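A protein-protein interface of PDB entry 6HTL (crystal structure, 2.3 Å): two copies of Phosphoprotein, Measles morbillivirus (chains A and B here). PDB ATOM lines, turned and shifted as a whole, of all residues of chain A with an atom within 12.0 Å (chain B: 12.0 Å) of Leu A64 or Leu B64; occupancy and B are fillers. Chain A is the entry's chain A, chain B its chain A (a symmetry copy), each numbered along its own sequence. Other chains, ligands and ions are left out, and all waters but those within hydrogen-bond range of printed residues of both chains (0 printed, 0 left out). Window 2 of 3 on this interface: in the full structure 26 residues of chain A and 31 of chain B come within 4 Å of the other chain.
The backbone carbonyl oxygen (O) of His B63 lies within hydrogen-bond range of the side-chain hydroxyl (OG) of Ser B66 (2.8 Å).
O of Glu A61 sits at hydrogen-bond distance from OG of Ser A65, at 3.1 Å.
Ser B56 touches Ile A57 (CB to CG2, 3.7 Å).
CD1 of Ile B57 touches CD1 of Ile A57, at 3.9 Å.
Ile A57 touches Leu B60 (O to CD1, 3.7 Å).
CD2 of Leu A60 touches CD2 of Leu B60, at 3.8 Å.
CD1 of Leu B60 touches CB of Glu A61, at 3.7 Å.
Leu A64 touches Leu B60.
His B63 touches Leu A64 (CB to CD2, 3.8 Å).
Leu A64 touches Leu B64 (CD1 to CD1, 3.8 Å).
Printed residues of chain B within 4 Å of Leu A64: Leu B60 (3.9 Å), His B63 (3.8 Å) and Leu B64 (3.8 Å).
Leu B64 touches one residue of chain A.
Leu A60 touches just one residue of chain B: Leu B60.
Of chain B, only Leu B60 comes within 4 Å of Glu A61.
No residue of chain B comes within 4 Å of Gly A62.
No residue of chain B comes within 4 Å of His A63.
Leu B60 touches four residues of chain A.
No residue of chain A comes within 4 Å of Glu B61.
No residue of chain A comes within 4 Å of Gly B62.
Of chain A, only Leu A64 comes within 4 Å of His B63.
No residue of chain A comes within 4 Å of Ser B66.
Of the printed residues of chain A, Ser B56 touches Ile A57.
Of the printed residues of chain A, Ile B57 touches Ile A57 (3.9 Å).
Printed residues of chain B within 4 Å of Ile A57: Ser B56 (3.7 Å), Ile B57 (3.9 Å) and Leu B60 (3.7 Å).
Thr B59 touches none of the printed residues of chain A.
Hydrophobic or aromatic side chains of chain A that line the printed part of chain B: Ile A57, Leu A60 and Leu A64.
Along chain A the printed residues that touch a printed residue of chain B span positions 57 to 64.
Among the printed residues, no Asp or Glu carboxylate lies within 4 Å of a Lys or Arg side-chain nitrogen of the other chain.
Glu A61 touches Leu B60, but with the chains exchanged Leu A60 does not touch Glu B61 (8.8 Å).
Leu A64 touches Leu B60, but with the chains exchanged Leu A60 does not touch Leu B64 (8.3 Å).
Leu A64 touches His B63, but with the chains exchanged His A63 does not touch Leu B64 (9.0 Å).
Leu B64 touches its own counterpart, Leu A64.
12 positions are printed for both chains.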
ATOM      1  N   ILE A  55      14.060  -4.134  -8.737  1.00  0.00           N
ATOM      2  CA  ILE A  55      12.673  -4.585  -8.697  1.00  0.00           C
ATOM      3  C   ILE A  55      11.935  -3.965  -7.498  1.00  0.00           C
ATOM      4  O   ILE A  55      10.812  -3.492  -7.670  1.00  0.00           O
ATOM      5  CB  ILE A  55      12.633  -6.151  -8.755  1.00  0.00           C
ATOM      6  CG1 ILE A  55      12.520  -6.634 -10.221  1.00  0.00           C
ATOM      7  CG2 ILE A  55      11.561  -6.795  -7.838  1.00  0.00           C
ATOM      8  CD1 ILE A  55      13.215  -7.951 -10.515  1.00  0.00           C
ATOM      9  N   SER A  56      12.577  -3.956  -6.302  1.00  0.00           N
ATOM     10  CA  SER A  56      12.051  -3.392  -5.060  1.00  0.00           C
ATOM     11  C   SER A  56      11.795  -1.896  -5.207  1.00  0.00           C
ATOM     12  O   SER A  56      10.761  -1.415  -4.753  1.00  0.00           O
ATOM     13  CB  SER A  56      13.016  -3.634  -3.907  1.00  0.00           C
ATOM     14  OG  SER A  56      13.027  -4.999  -3.532  1.00  0.00           O
ATOM     15  N   ILE A  57      12.721  -1.173  -5.864  1.00  0.00           N
ATOM     16  CA  ILE A  57      12.606   0.262  -6.119  1.00  0.00           C
ATOM     17  C   ILE A  57      11.474   0.519  -7.119  1.00  0.00           C
ATOM     18  O   ILE A  57      10.717   1.475  -6.940  1.00  0.00           O
ATOM     19  CB  ILE A  57      13.971   0.906  -6.515  1.00  0.00           C
ATOM     20  CG1 ILE A  57      14.990   0.750  -5.365  1.00  0.00           C
ATOM     21  CG2 ILE A  57      13.805   2.394  -6.866  1.00  0.00           C
ATOM     22  CD1 ILE A  57      16.408   0.786  -5.762  1.00  0.00           C
ATOM     23  N   SER A  58      11.322  -0.371  -8.123  1.00  0.00           N
ATOM     24  CA  SER A  58      10.253  -0.293  -9.131  1.00  0.00           C
ATOM     25  C   SER A  58       8.873  -0.548  -8.518  1.00  0.00           C
ATOM     26  O   SER A  58       7.902   0.068  -8.953  1.00  0.00           O
ATOM     27  CB  SER A  58      10.520  -1.248 -10.292  1.00  0.00           C
ATOM     28  OG  SER A  58      11.467  -0.677 -11.179  1.00  0.00           O
ATOM     29  N   THR A  59       8.804  -1.438  -7.497  1.00  0.00           N
ATOM     30  CA  THR A  59       7.603  -1.772  -6.731  1.00  0.00           C
ATOM     31  C   THR A  59       7.218  -0.562  -5.860  1.00  0.00           C
ATOM     32  O   THR A  59       6.036  -0.222  -5.770  1.00  0.00           O
ATOM     33  CB  THR A  59       7.847  -3.059  -5.921  1.00  0.00           C
ATOM     34  OG1 THR A  59       7.904  -4.158  -6.829  1.00  0.00           O
ATOM     35  CG2 THR A  59       6.768  -3.328  -4.877  1.00  0.00           C
ATOM     36  N   LEU A  60       8.225   0.087  -5.237  1.00  0.00           N
ATOM     37  CA  LEU A  60       8.066   1.284  -4.415  1.00  0.00           C
ATOM     38  C   LEU A  60       7.551   2.438  -5.276  1.00  0.00           C
ATOM     39  O   LEU A  60       6.748   3.234  -4.794  1.00  0.00           O
ATOM     40  CB  LEU A  60       9.404   1.670  -3.768  1.00  0.00           C
ATOM     41  CG  LEU A  60       9.495   1.507  -2.266  1.00  0.00           C
ATOM     42  CD1 LEU A  60       9.943   0.108  -1.892  1.00  0.00           C
ATOM     43  CD2 LEU A  60      10.460   2.503  -1.681  1.00  0.00           C
ATOM     44  N   GLU A  61       7.995   2.509  -6.553  1.00  0.00           N
ATOM     45  CA  GLU A  61       7.561   3.515  -7.528  1.00  0.00           C
ATOM     46  C   GLU A  61       6.062   3.338  -7.834  1.00  0.00           C
ATOM     47  O   GLU A  61       5.330   4.330  -7.908  1.00  0.00           O
ATOM     48  CB  GLU A  61       8.393   3.425  -8.821  1.00  0.00           C
ATOM     49  N   GLY A  62       5.632   2.082  -7.977  1.00  0.00           N
ATOM     50  CA  GLY A  62       4.244   1.721  -8.235  1.00  0.00           C
ATOM     51  C   GLY A  62       3.336   2.027  -7.058  1.00  0.00           C
ATOM     52  O   GLY A  62       2.315   2.703  -7.224  1.00  0.00           O
ATOM     53  N   HIS A  63       3.722   1.555  -5.853  1.00  0.00           N
ATOM     54  CA  HIS A  63       2.975   1.769  -4.608  1.00  0.00           C
ATOM     55  C   HIS A  63       2.839   3.254  -4.238  1.00  0.00           C
ATOM     56  O   HIS A  63       1.866   3.617  -3.577  1.00  0.00           O
ATOM     57  CB  HIS A  63       3.573   0.954  -3.448  1.00  0.00           C
ATOM     58  N   LEU A  64       3.786   4.106  -4.685  1.00  0.00           N
ATOM     59  CA  LEU A  64       3.759   5.551  -4.449  1.00  0.00           C
ATOM     60  C   LEU A  64       2.792   6.235  -5.425  1.00  0.00           C
ATOM     61  O   LEU A  64       2.058   7.140  -5.019  1.00  0.00           O
ATOM     62  CB  LEU A  64       5.170   6.155  -4.554  1.00  0.00           C
ATOM     63  CG  LEU A  64       5.344   7.640  -4.226  1.00  0.00           C
ATOM     64  CD1 LEU A  64       5.153   7.913  -2.746  1.00  0.00           C
ATOM     65  CD2 LEU A  64       6.718   8.118  -4.639  1.00  0.00           C
ATOM     66  N   SER A  65       2.766   5.782  -6.698  1.00  0.00           N
ATOM     67  CA  SER A  65       1.880   6.315  -7.738  1.00  0.00           C
ATOM     68  C   SER A  65       0.430   5.791  -7.578  1.00  0.00           C
ATOM     69  O   SER A  65      -0.168   5.258  -8.521  1.00  0.00           O
ATOM     70  CB  SER A  65       2.451   6.034  -9.129  1.00  0.00           C
ATOM     71  OG  SER A  65       2.598   4.644  -9.368  1.00  0.00           O
ATOM     72  N   SER A  66      -0.117   5.948  -6.353  1.00  0.00           N
ATOM     73  CA  SER A  66      -1.470   5.565  -5.941  1.00  0.00           C
ATOM     74  C   SER A  66      -1.888   6.335  -4.679  1.00  0.00           C
ATOM     75  O   SER A  66      -1.314   7.378  -4.352  1.00  0.00           O
ATOM     76  CB  SER A  66      -1.564   4.060  -5.699  1.00  0.00           C
ATOM     77  OG  SER A  66      -0.689   3.636  -4.667  1.00  0.00           O
ATOM     78  N   ILE B  55      19.209   6.808 -10.468  1.00  0.00           N
ATOM     79  CA  ILE B  55      18.216   7.565 -11.222  1.00  0.00           C
ATOM     80  C   ILE B  55      16.797   7.256 -10.715  1.00  0.00           C
ATOM     81  O   ILE B  55      16.017   8.188 -10.524  1.00  0.00           O
ATOM     82  CB  ILE B  55      18.433   7.325 -12.755  1.00  0.00           C
ATOM     83  CG1 ILE B  55      19.379   8.400 -13.343  1.00  0.00           C
ATOM     84  CG2 ILE B  55      17.120   7.188 -13.571  1.00  0.00           C
ATOM     85  CD1 ILE B  55      20.263   7.921 -14.480  1.00  0.00           C
ATOM     86  N   SER B  56      16.482   5.955 -10.485  1.00  0.00           N
ATOM     87  CA  SER B  56      15.200   5.468  -9.980  1.00  0.00           C
ATOM     88  C   SER B  56      14.909   6.035  -8.595  1.00  0.00           C
ATOM     89  O   SER B  56      13.780   6.443  -8.337  1.00  0.00           O
ATOM     90  CB  SER B  56      15.186   3.946  -9.922  1.00  0.00           C
ATOM     91  OG  SER B  56      15.129   3.389 -11.221  1.00  0.00           O
ATOM     92  N   ILE B  57      15.931   6.085  -7.720  1.00  0.00           N
ATOM     93  CA  ILE B  57      15.824   6.632  -6.369  1.00  0.00           C
ATOM     94  C   ILE B  57      15.610   8.148  -6.442  1.00  0.00           C
ATOM     95  O   ILE B  57      14.805   8.681  -5.676  1.00  0.00           O
ATOM     96  CB  ILE B  57      17.009   6.194  -5.455  1.00  0.00           C
ATOM     97  CG1 ILE B  57      17.026   4.658  -5.301  1.00  0.00           C
ATOM     98  CG2 ILE B  57      16.920   6.855  -4.070  1.00  0.00           C
ATOM     99  CD1 ILE B  57      18.334   4.066  -4.965  1.00  0.00           C
ATOM    100  N   SER B  58      16.278   8.821  -7.404  1.00  0.00           N
ATOM    101  CA  SER B  58      16.141  10.268  -7.637  1.00  0.00           C
ATOM    102  C   SER B  58      14.749  10.629  -8.163  1.00  0.00           C
ATOM    103  O   SER B  58      14.235  11.691  -7.815  1.00  0.00           O
ATOM    104  CB  SER B  58      17.230  10.779  -8.575  1.00  0.00           C
ATOM    105  OG  SER B  58      18.440  10.959  -7.858  1.00  0.00           O
ATOM    106  N   THR B  59      14.143   9.732  -8.980  1.00  0.00           N
ATOM    107  CA  THR B  59      12.793   9.851  -9.532  1.00  0.00           C
ATOM    108  C   THR B  59      11.774   9.680  -8.390  1.00  0.00           C
ATOM    109  O   THR B  59      10.794  10.427  -8.327  1.00  0.00           O
ATOM    110  CB  THR B  59      12.611   8.836 -10.676  1.00  0.00           C
ATOM    111  OG1 THR B  59      13.398   9.263 -11.787  1.00  0.00           O
ATOM    112  CG2 THR B  59      11.161   8.681 -11.120  1.00  0.00           C
ATOM    113  N   LEU B  60      12.022   8.705  -7.490  1.00  0.00           N
ATOM    114  CA  LEU B  60      11.204   8.426  -6.313  1.00  0.00           C
ATOM    115  C   LEU B  60      11.237   9.624  -5.364  1.00  0.00           C
ATOM    116  O   LEU B  60      10.219   9.927  -4.746  1.00  0.00           O
ATOM    117  CB  LEU B  60      11.717   7.172  -5.591  1.00  0.00           C
ATOM    118  CG  LEU B  60      10.816   5.957  -5.635  1.00  0.00           C
ATOM    119  CD1 LEU B  60      11.087   5.117  -6.867  1.00  0.00           C
ATOM    120  CD2 LEU B  60      11.013   5.104  -4.409  1.00  0.00           C
ATOM    121  N   GLU B  61      12.398  10.315  -5.273  1.00  0.00           N
ATOM    122  CA  GLU B  61      12.586  11.518  -4.456  1.00  0.00           C
ATOM    123  C   GLU B  61      11.701  12.660  -4.991  1.00  0.00           C
ATOM    124  O   GLU B  61      11.077  13.374  -4.201  1.00  0.00           O
ATOM    125  CB  GLU B  61      14.066  11.944  -4.433  1.00  0.00           C
ATOM    126  N   GLY B  62      11.644  12.790  -6.319  1.00  0.00           N
ATOM    127  CA  GLY B  62      10.834  13.790  -7.004  1.00  0.00           C
ATOM    128  C   GLY B  62       9.346  13.543  -6.842  1.00  0.00           C
ATOM    129  O   GLY B  62       8.610  14.445  -6.430  1.00  0.00           O
ATOM    130  N   HIS B  63       8.900  12.302  -7.137  1.00  0.00           N
ATOM    131  CA  HIS B  63       7.498  11.883  -7.024  1.00  0.00           C
ATOM    132  C   HIS B  63       6.956  11.985  -5.590  1.00  0.00           C
ATOM    133  O   HIS B  63       5.753  12.176  -5.419  1.00  0.00           O
ATOM    134  CB  HIS B  63       7.284  10.475  -7.606  1.00  0.00           C
ATOM    135  N   LEU B  64       7.839  11.889  -4.572  1.00  0.00           N
ATOM    136  CA  LEU B  64       7.471  12.016  -3.160  1.00  0.00           C
ATOM    137  C   LEU B  64       7.308  13.493  -2.779  1.00  0.00           C
ATOM    138  O   LEU B  64       6.377  13.831  -2.043  1.00  0.00           O
ATOM    139  CB  LEU B  64       8.505  11.322  -2.257  1.00  0.00           C
ATOM    140  CG  LEU B  64       8.220  11.260  -0.754  1.00  0.00           C
ATOM    141  CD1 LEU B  64       7.067  10.325  -0.440  1.00  0.00           C
ATOM    142  CD2 LEU B  64       9.446  10.795   0.001  1.00  0.00           C
ATOM    143  N   SER B  65       8.188  14.374  -3.304  1.00  0.00           N
ATOM    144  CA  SER B  65       8.147  15.819  -3.054  1.00  0.00           C
ATOM    145  C   SER B  65       7.037  16.511  -3.887  1.00  0.00           C
ATOM    146  O   SER B  65       7.287  17.491  -4.601  1.00  0.00           O
ATOM    147  CB  SER B  65       9.524  16.445  -3.283  1.00  0.00           C
ATOM    148  OG  SER B  65       9.974  16.256  -4.614  1.00  0.00           O
ATOM    149  N   SER B  66       5.804  15.970  -3.784  1.00  0.00           N
ATOM    150  CA  SER B  66       4.582  16.440  -4.440  1.00  0.00           C
ATOM    151  C   SER B  66       3.339  15.910  -3.710  1.00  0.00           C
ATOM    152  O   SER B  66       3.410  15.509  -2.545  1.00  0.00           O
ATOM    153  CB  SER B  66       4.553  16.021  -5.909  1.00  0.00           C
ATOM    154  OG  SER B  66       4.577  14.611  -6.056  1.00  0.00           O
